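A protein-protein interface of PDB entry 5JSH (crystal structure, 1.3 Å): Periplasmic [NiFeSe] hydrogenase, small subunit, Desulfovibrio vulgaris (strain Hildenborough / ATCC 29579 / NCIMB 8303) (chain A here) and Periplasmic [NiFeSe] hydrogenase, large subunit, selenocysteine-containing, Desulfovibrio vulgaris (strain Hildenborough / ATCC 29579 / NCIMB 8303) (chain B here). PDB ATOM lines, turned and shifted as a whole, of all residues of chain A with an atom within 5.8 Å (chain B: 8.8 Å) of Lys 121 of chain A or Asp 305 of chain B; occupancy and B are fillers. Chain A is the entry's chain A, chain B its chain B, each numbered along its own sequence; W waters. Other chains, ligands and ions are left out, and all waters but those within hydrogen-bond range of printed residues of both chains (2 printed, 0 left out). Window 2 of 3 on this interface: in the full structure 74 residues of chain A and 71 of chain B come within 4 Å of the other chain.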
ATOM      1  N   PRO A 115      17.742  25.288   9.253  1.00  0.00           N
ATOM      2  CA  PRO A 115      17.180  25.277  10.609  1.00  0.00           C
ATOM      3  C   PRO A 115      17.406  23.954  11.313  1.00  0.00           C
ATOM      4  O   PRO A 115      17.044  22.896  10.786  1.00  0.00           O
ATOM      5  CB  PRO A 115      15.697  25.554  10.362  1.00  0.00           C
ATOM      6  CG  PRO A 115      15.427  24.944   9.004  1.00  0.00           C
ATOM      7  CD  PRO A 115      16.714  25.069   8.220  1.00  0.00           C
ATOM      8  N   GLU A 117      16.400  23.264  14.691  1.00  0.00           N
ATOM      9  CA  GLU A 117      15.456  22.924  15.748  1.00  0.00           C
ATOM     10  C   GLU A 117      14.483  21.851  15.274  1.00  0.00           C
ATOM     11  O   GLU A 117      14.289  21.624  14.078  1.00  0.00           O
ATOM     12  CB  GLU A 117      14.666  24.152  16.197  1.00  0.00           C
ATOM     13  CG  GLU A 117      15.470  25.149  16.990  1.00  0.00           C
ATOM     14  CD  GLU A 117      15.935  24.613  18.322  1.00  0.00           C
ATOM     15  OE1 GLU A 117      15.176  23.850  18.952  1.00  0.00           O
ATOM     16  OE2 GLU A 117      17.064  24.955  18.732  1.00  0.00           O
ATOM     17  N   ALA A 118      13.865  21.177  16.242  1.00  0.00           N
ATOM     18  CA  ALA A 118      12.844  20.178  15.957  1.00  0.00           C
ATOM     19  C   ALA A 118      13.354  19.121  14.983  1.00  0.00           C
ATOM     20  O   ALA A 118      12.663  18.714  14.054  1.00  0.00           O
ATOM     21  CB  ALA A 118      11.561  20.839  15.444  1.00  0.00           C
ATOM     22  N   ASP A 119      14.600  18.697  15.177  1.00  0.00           N
ATOM     23  CA  ASP A 119      15.196  17.631  14.371  1.00  0.00           C
ATOM     24  C   ASP A 119      15.135  17.935  12.875  1.00  0.00           C
ATOM     25  O   ASP A 119      14.985  17.035  12.055  1.00  0.00           O
ATOM     26  CB  ASP A 119      14.549  16.278  14.684  1.00  0.00           C
ATOM     27  CG  ASP A 119      15.328  15.122  14.130  1.00  0.00           C
ATOM     28  OD1 ASP A 119      16.575  15.195  14.101  1.00  0.00           O
ATOM     29  OD2 ASP A 119      14.690  14.137  13.715  1.00  0.00           O
ATOM     30  N   GLY A 120      15.252  19.206  12.503  1.00  0.00           N
ATOM     31  CA  GLY A 120      15.314  19.601  11.106  1.00  0.00           C
ATOM     32  C   GLY A 120      13.971  19.850  10.452  1.00  0.00           C
ATOM     33  O   GLY A 120      13.935  20.202   9.263  1.00  0.00           O
ATOM     34  N   LYS A 121      12.870  19.668  11.184  1.00  0.00           N
ATOM     35  CA  LYS A 121      11.538  19.640  10.588  1.00  0.00           C
ATOM     36  C   LYS A 121      11.071  20.980  10.042  1.00  0.00           C
ATOM     37  O   LYS A 121      10.068  21.012   9.321  1.00  0.00           O
ATOM     38  CB  LYS A 121      10.512  19.154  11.619  1.00  0.00           C
ATOM     39  CG  LYS A 121      10.543  17.671  11.881  1.00  0.00           C
ATOM     40  CD  LYS A 121       9.410  17.252  12.826  1.00  0.00           C
ATOM     41  CE  LYS A 121       9.529  15.810  13.220  1.00  0.00           C
ATOM     42  NZ  LYS A 121       8.393  15.430  14.097  1.00  0.00           N
ATOM     43  N   TYR A 122      11.756  22.086  10.347  1.00  0.00           N
ATOM     44  CA  TYR A 122      11.333  23.373   9.802  1.00  0.00           C
ATOM     45  C   TYR A 122      11.769  23.582   8.349  1.00  0.00           C
ATOM     46  O   TYR A 122      11.408  24.604   7.757  1.00  0.00           O
ATOM     47  CB  TYR A 122      11.796  24.524  10.694  1.00  0.00           C
ATOM     48  CG  TYR A 122      11.069  24.626  12.022  1.00  0.00           C
ATOM     49  CD1 TYR A 122       9.698  24.880  12.074  1.00  0.00           C
ATOM     50  CD2 TYR A 122      11.754  24.506  13.227  1.00  0.00           C
ATOM     51  CE1 TYR A 122       9.041  25.006  13.291  1.00  0.00           C
ATOM     52  CE2 TYR A 122      11.114  24.641  14.438  1.00  0.00           C
ATOM     53  CZ  TYR A 122       9.749  24.884  14.468  1.00  0.00           C
ATOM     54  OH  TYR A 122       9.111  25.010  15.680  1.00  0.00           O
ATOM     55  N   CYS A 123      12.478  22.622   7.737  1.00  0.00           N
ATOM     56  CA  CYS A 123      12.765  22.715   6.303  1.00  0.00           C
ATOM     57  C   CYS A 123      12.928  21.312   5.732  1.00  0.00           C
ATOM     58  O   CYS A 123      14.008  20.710   5.833  1.00  0.00           O
ATOM     59  CB  CYS A 123      14.003  23.546   6.024  1.00  0.00           C
ATOM     60  SG  CYS A 123      14.205  23.870   4.273  1.00  0.00           S
ATOM     61  N   ILE A 124      11.866  20.812   5.110  1.00  0.00           N
ATOM     62  CA  ILE A 124      11.904  19.542   4.382  1.00  0.00           C
ATOM     63  C   ILE A 124      12.022  19.860   2.899  1.00  0.00           C
ATOM     64  O   ILE A 124      11.182  20.583   2.353  1.00  0.00           O
ATOM     65  CB  ILE A 124      10.659  18.686   4.666  1.00  0.00           C
ATOM     66  CG1 ILE A 124      10.534  18.387   6.170  1.00  0.00           C
ATOM     67  CG2 ILE A 124      10.714  17.394   3.842  1.00  0.00           C
ATOM     68  CD1 ILE A 124      11.715  17.635   6.754  1.00  0.00           C
ATOM     69  N   SER A 134      15.380  16.434   5.220  1.00  0.00           N
ATOM     70  CA  SER A 134      15.452  17.794   5.722  1.00  0.00           C
ATOM     71  C   SER A 134      16.659  18.513   5.119  1.00  0.00           C
ATOM     72  O   SER A 134      17.569  17.890   4.561  1.00  0.00           O
ATOM     73  CB  SER A 134      15.593  17.784   7.242  1.00  0.00           C
ATOM     74  OG  SER A 134      16.864  17.253   7.616  1.00  0.00           O
ATOM     75  N   GLY B  46       3.220  22.258   2.844  1.00  0.00           N
ATOM     76  CA  GLY B  46       4.261  23.266   2.797  1.00  0.00           C
ATOM     77  C   GLY B  46       5.285  22.946   3.862  1.00  0.00           C
ATOM     78  O   GLY B  46       4.978  22.982   5.057  1.00  0.00           O
ATOM     79  N   GLY B  47       6.489  22.564   3.454  1.00  0.00           N
ATOM     80  CA  GLY B  47       7.453  21.971   4.355  1.00  0.00           C
ATOM     81  C   GLY B  47       8.535  22.870   4.921  1.00  0.00           C
ATOM     82  O   GLY B  47       9.450  22.348   5.565  1.00  0.00           O
ATOM     83  N   MET B  48       8.464  24.192   4.738  1.00  0.00           N
ATOM     84  CA  MET B  48       9.487  25.091   5.266  1.00  0.00           C
ATOM     85  C   MET B  48       8.830  26.278   5.949  1.00  0.00           C
ATOM     86  O   MET B  48       7.912  26.890   5.399  1.00  0.00           O
ATOM     87  CB  MET B  48      10.441  25.542   4.147  1.00  0.00           C
ATOM     88  CG  MET B  48      11.622  26.393   4.640  1.00  0.00           C
ATOM     89  SD  MET B  48      11.262  28.161   4.853  1.00  0.00           S
ATOM     90  CE  MET B  48      11.295  28.712   3.169  1.00  0.00           C
ATOM     91  N   TYR B  49       9.303  26.595   7.154  1.00  0.00           N
ATOM     92  CA  TYR B  49       8.771  27.685   7.954  1.00  0.00           C
ATOM     93  C   TYR B  49       9.895  28.610   8.406  1.00  0.00           C
ATOM     94  O   TYR B  49      10.980  28.147   8.766  1.00  0.00           O
ATOM     95  CB  TYR B  49       8.093  27.090   9.192  1.00  0.00           C
ATOM     96  CG  TYR B  49       7.604  28.080  10.226  1.00  0.00           C
ATOM     97  CD1 TYR B  49       6.379  28.728  10.088  1.00  0.00           C
ATOM     98  CD2 TYR B  49       8.359  28.349  11.365  1.00  0.00           C
ATOM     99  CE1 TYR B  49       5.929  29.629  11.047  1.00  0.00           C
ATOM    100  CE2 TYR B  49       7.918  29.250  12.326  1.00  0.00           C
ATOM    101  CZ  TYR B  49       6.690  29.880  12.169  1.00  0.00           C
ATOM    102  OH  TYR B  49       6.198  30.773  13.098  1.00  0.00           O
ATOM    103  N   SER B 284      -2.505  21.905  10.414  1.00  0.00           N
ATOM    104  CA  SER B 284      -1.308  22.727  10.271  1.00  0.00           C
ATOM    105  C   SER B 284      -0.460  22.628  11.538  1.00  0.00           C
ATOM    106  O   SER B 284      -0.977  22.382  12.631  1.00  0.00           O
ATOM    107  CB  SER B 284      -1.706  24.182  10.028  1.00  0.00           C
ATOM    108  OG  SER B 284      -2.631  24.285   8.961  1.00  0.00           O
ATOM    109  N   TRP B 285       0.856  22.797  11.386  1.00  0.00           N
ATOM    110  CA  TRP B 285       1.796  22.647  12.505  1.00  0.00           C
ATOM    111  C   TRP B 285       1.855  23.902  13.386  1.00  0.00           C
ATOM    112  O   TRP B 285       2.880  24.578  13.505  1.00  0.00           O
ATOM    113  CB  TRP B 285       3.175  22.261  11.981  1.00  0.00           C
ATOM    114  CG  TRP B 285       3.258  20.843  11.485  1.00  0.00           C
ATOM    115  CD1 TRP B 285       2.924  19.723  12.175  1.00  0.00           C
ATOM    116  CD2 TRP B 285       3.724  20.402  10.202  1.00  0.00           C
ATOM    117  NE1 TRP B 285       3.143  18.610  11.406  1.00  0.00           N
ATOM    118  CE2 TRP B 285       3.634  19.000  10.185  1.00  0.00           C
ATOM    119  CE3 TRP B 285       4.228  21.057   9.070  1.00  0.00           C
ATOM    120  CZ2 TRP B 285       4.028  18.237   9.083  1.00  0.00           C
ATOM    121  CZ3 TRP B 285       4.602  20.302   7.971  1.00  0.00           C
ATOM    122  CH2 TRP B 285       4.501  18.906   7.984  1.00  0.00           C
ATOM    123  N   PHE B 286       0.713  24.208  14.002  1.00  0.00           N
ATOM    124  CA  PHE B 286       0.566  25.321  14.940  1.00  0.00           C
ATOM    125  C   PHE B 286      -0.267  24.867  16.131  1.00  0.00           C
ATOM    126  O   PHE B 286      -1.060  23.930  16.031  1.00  0.00           O
ATOM    127  CB  PHE B 286      -0.076  26.543  14.267  1.00  0.00           C
ATOM    128  CG  PHE B 286       0.747  27.050  13.138  1.00  0.00           C
ATOM    129  CD1 PHE B 286       1.891  27.801  13.387  1.00  0.00           C
ATOM    130  CD2 PHE B 286       0.452  26.702  11.836  1.00  0.00           C
ATOM    131  CE1 PHE B 286       2.699  28.212  12.347  1.00  0.00           C
ATOM    132  CE2 PHE B 286       1.250  27.131  10.801  1.00  0.00           C
ATOM    133  CZ  PHE B 286       2.377  27.877  11.061  1.00  0.00           C
ATOM    134  N   ALA B 287      -0.092  25.552  17.260  1.00  0.00           N
ATOM    135  CA  ALA B 287      -0.739  25.143  18.497  1.00  0.00           C
ATOM    136  C   ALA B 287      -2.255  25.150  18.334  1.00  0.00           C
ATOM    137  O   ALA B 287      -2.836  26.074  17.757  1.00  0.00           O
ATOM    138  CB  ALA B 287      -0.335  26.079  19.632  1.00  0.00           C
ATOM    139  N   PRO B 302       4.282  27.922  16.417  1.00  0.00           N
ATOM    140  CA  PRO B 302       4.579  26.673  15.709  1.00  0.00           C
ATOM    141  C   PRO B 302       4.481  25.458  16.617  1.00  0.00           C
ATOM    142  O   PRO B 302       4.755  25.517  17.819  1.00  0.00           O
ATOM    143  CB  PRO B 302       6.002  26.886  15.170  1.00  0.00           C
ATOM    144  CG  PRO B 302       6.548  28.039  15.881  1.00  0.00           C
ATOM    145  CD  PRO B 302       5.411  28.866  16.388  1.00  0.00           C
ATOM    146  N   ALA B 303       4.032  24.353  16.021  1.00  0.00           N
ATOM    147  CA  ALA B 303       3.911  23.065  16.701  1.00  0.00           C
ATOM    148  C   ALA B 303       4.302  21.972  15.721  1.00  0.00           C
ATOM    149  O   ALA B 303       3.457  21.226  15.215  1.00  0.00           O
ATOM    150  CB  ALA B 303       2.492  22.866  17.232  1.00  0.00           C
ATOM    151  N   PRO B 304       5.600  21.842  15.437  1.00  0.00           N
ATOM    152  CA  PRO B 304       6.040  20.951  14.353  1.00  0.00           C
ATOM    153  C   PRO B 304       5.842  19.478  14.630  1.00  0.00           C
ATOM    154  O   PRO B 304       5.955  18.685  13.691  1.00  0.00           O
ATOM    155  CB  PRO B 304       7.527  21.289  14.204  1.00  0.00           C
ATOM    156  CG  PRO B 304       7.926  21.766  15.556  1.00  0.00           C
ATOM    157  CD  PRO B 304       6.731  22.532  16.068  1.00  0.00           C
ATOM    158  N   ASP B 305       5.570  19.088  15.870  1.00  0.00           N
ATOM    159  CA  ASP B 305       5.342  17.693  16.219  1.00  0.00           C
ATOM    160  C   ASP B 305       3.860  17.356  16.398  1.00  0.00           C
ATOM    161  O   ASP B 305       3.532  16.227  16.786  1.00  0.00           O
ATOM    162  CB  ASP B 305       6.117  17.341  17.495  1.00  0.00           C
ATOM    163  CG  ASP B 305       7.620  17.476  17.322  1.00  0.00           C
ATOM    164  OD1 ASP B 305       8.134  17.069  16.268  1.00  0.00           O
ATOM    165  OD2 ASP B 305       8.290  18.004  18.232  1.00  0.00           O
ATOM    166  N   LYS B 306       2.950  18.288  16.111  1.00  0.00           N
ATOM    167  CA  LYS B 306       1.538  18.044  16.407  1.00  0.00           C
ATOM    168  C   LYS B 306       0.978  16.921  15.540  1.00  0.00           C
ATOM    169  O   LYS B 306       1.059  16.976  14.306  1.00  0.00           O
ATOM    170  CB  LYS B 306       0.710  19.312  16.191  1.00  0.00           C
ATOM    171  CG  LYS B 306      -0.754  19.145  16.678  1.00  0.00           C
ATOM    172  CD  LYS B 306      -1.584  20.425  16.536  1.00  0.00           C
ATOM    173  CE  LYS B 306      -1.935  20.706  15.094  1.00  0.00           C
ATOM    174  NZ  LYS B 306      -2.744  21.946  14.951  1.00  0.00           N
ATOM    175  N   ALA B 307       0.353  15.931  16.184  1.00  0.00           N
ATOM    176  CA  ALA B 307      -0.185  14.779  15.473  1.00  0.00           C
ATOM    177  C   ALA B 307      -1.281  15.195  14.500  1.00  0.00           C
ATOM    178  O   ALA B 307      -2.101  16.068  14.795  1.00  0.00           O
ATOM    179  CB  ALA B 307      -0.760  13.773  16.472  1.00  0.00           C
ATOM    180  N   GLY B 308      -1.295  14.548  13.332  1.00  0.00           N
ATOM    181  CA  GLY B 308      -2.323  14.748  12.332  1.00  0.00           C
ATOM    182  C   GLY B 308      -2.083  15.911  11.390  1.00  0.00           C
ATOM    183  O   GLY B 308      -2.654  15.935  10.292  1.00  0.00           O
ATOM    184  N   ALA B 309      -1.237  16.861  11.766  1.00  0.00           N
ATOM    185  CA  ALA B 309      -0.990  18.000  10.900  1.00  0.00           C
ATOM    186  C   ALA B 309      -0.031  17.611   9.787  1.00  0.00           C
ATOM    187  O   ALA B 309       0.785  16.701   9.929  1.00  0.00           O
ATOM    188  CB  ALA B 309      -0.408  19.149  11.715  1.00  0.00           C
ATOM    189  N   TYR B 310      -0.105  18.346   8.667  1.00  0.00           N
ATOM    190  CA  TYR B 310       0.737  17.993   7.530  1.00  0.00           C
ATOM    191  C   TYR B 310       1.262  19.198   6.757  1.00  0.00           C
ATOM    192  O   TYR B 310       1.759  19.027   5.636  1.00  0.00           O
ATOM    193  CB  TYR B 310       0.040  16.983   6.599  1.00  0.00           C
ATOM    194  CG  TYR B 310      -1.244  17.435   5.914  1.00  0.00           C
ATOM    195  CD1 TYR B 310      -1.211  18.103   4.700  1.00  0.00           C
ATOM    196  CD2 TYR B 310      -2.498  17.105   6.442  1.00  0.00           C
ATOM    197  CE1 TYR B 310      -2.384  18.484   4.054  1.00  0.00           C
ATOM    198  CE2 TYR B 310      -3.666  17.471   5.805  1.00  0.00           C
ATOM    199  CZ  TYR B 310      -3.614  18.155   4.603  1.00  0.00           C
ATOM    200  OH  TYR B 310      -4.793  18.517   3.965  1.00  0.00           O
ATOM    201  N   SER B 311       1.196  20.402   7.322  1.00  0.00           N
ATOM    202  CA  SER B 311       1.674  21.562   6.582  1.00  0.00           C
ATOM    203  C   SER B 311       1.967  22.719   7.528  1.00  0.00           C
ATOM    204  O   SER B 311       1.335  22.842   8.578  1.00  0.00           O
ATOM    205  CB  SER B 311       0.591  22.012   5.592  1.00  0.00           C
ATOM    206  OG  SER B 311       1.109  23.035   4.761  1.00  0.00           O
ATOM    207  N   PHE B 312       2.911  23.585   7.130  1.00  0.00           N
ATOM    208  CA  PHE B 312       3.131  24.866   7.797  1.00  0.00           C
ATOM    209  C   PHE B 312       2.234  25.985   7.255  1.00  0.00           C
ATOM    210  O   PHE B 312       2.323  27.125   7.731  1.00  0.00           O
ATOM    211  CB  PHE B 312       4.608  25.283   7.714  1.00  0.00           C
ATOM    212  CG  PHE B 312       5.534  24.467   8.578  1.00  0.00           C
ATOM    213  CD1 PHE B 312       5.438  24.502   9.969  1.00  0.00           C
ATOM    214  CD2 PHE B 312       6.532  23.684   8.011  1.00  0.00           C
ATOM    215  CE1 PHE B 312       6.303  23.764  10.775  1.00  0.00           C
ATOM    216  CE2 PHE B 312       7.406  22.939   8.809  1.00  0.00           C
ATOM    217  CZ  PHE B 312       7.292  22.975  10.199  1.00  0.00           C
HETATM  218  O   HOH W   1      10.714  17.145  16.244  1.00  0.00           O
HETATM  219  O   HOH W   2       5.761  16.084  12.886  1.00  0.00           O
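NZ of Lys 121 of chain A is in salt-bridge range of OD1 of Asp 305 of chain B.
O of Tyr 122 of chain A sits at hydrogen-bond distance from N of Tyr 49 of chain B, 3.0 Å away.
N of Ile 124 of chain A is in hydrogen-bond range of O of Gly 47 of chain B (2.9 Å).
The backbone carbonyl oxygen of Gly 46 of chain B sits at hydrogen-bond distance from the backbone NH of Phe 312 of chain B (3.0 Å).
Among the printed residues, pairs that only touch across the chains: Tyr 122 of chain A with Met 48 of chain B (3.2 Å), Lys 121 of chain A with Phe 312 of chain B (3.3 Å), Cys 123 of chain A with Gly 47 of chain B (3.4 Å), Tyr 122 of chain A with Pro 304 of chain B (3.5 Å), Tyr 122 of chain A with Phe 312 of chain B (3.6 Å), Cys 123 of chain A with Met 48 of chain B (3.6 Å), Tyr 122 of chain A with Pro 302 of chain B (3.7 Å), Tyr 122 of chain A with Gly 47 of chain B (3.7 Å), Ala 118 of chain A with Pro 304 of chain B (3.8 Å) and Lys 121 of chain A with Pro 304 of chain B (3.8 Å).
Asp 305 of chain B touches just one residue of chain A: Lys 121 (2.7 Å).
Gly 120 of chain A touches none of the printed residues of chain B.
Of the printed residues of chain B, Ala 118 of chain A touches Pro 304.
Of the printed residues of chain A, Gly 47 of chain B touches Tyr 122 (3.7 Å), Cys 123 (3.4 Å) and Ile 124 (2.9 Å).
The nearest residue of chain B that does not touch Lys 121 of chain A is Gly 47 of chain B (4.03 Å).
The nearest residue of chain A that does not touch Asp 305 of chain B is Ala 118 of chain A (5.1 Å).
Printed residues of chain B that touch a printed residue of chain A: Gly 47, Met 48, Tyr 49, Pro 302, Pro 304, Asp 305 and Phe 312.
Of the 10 printed residues of chain A, 5 touch a printed residue of chain B.
Printed residues of chain A that touch a printed residue of chain B: Ala 118, Lys 121, Tyr 122, Cys 123 and Ile 124.
Hydrophobic or aromatic side chains of chain A that line the printed part of chain B: Ala 118, Tyr 122 and Ile 124.
Among the printed residues, 13 pairs touch across the chains.
Water W1 bridges OD1 of Asp 305 of chain B (2.6 Å) and O of Ala 118 of chain A (3.3 Å).
Water W2 lies within hydrogen-bond range of the backbone carbonyl oxygen of Pro 304 of chain B (2.7 Å) and the side-chain amino group of Lys 121 of chain A (3.0 Å).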
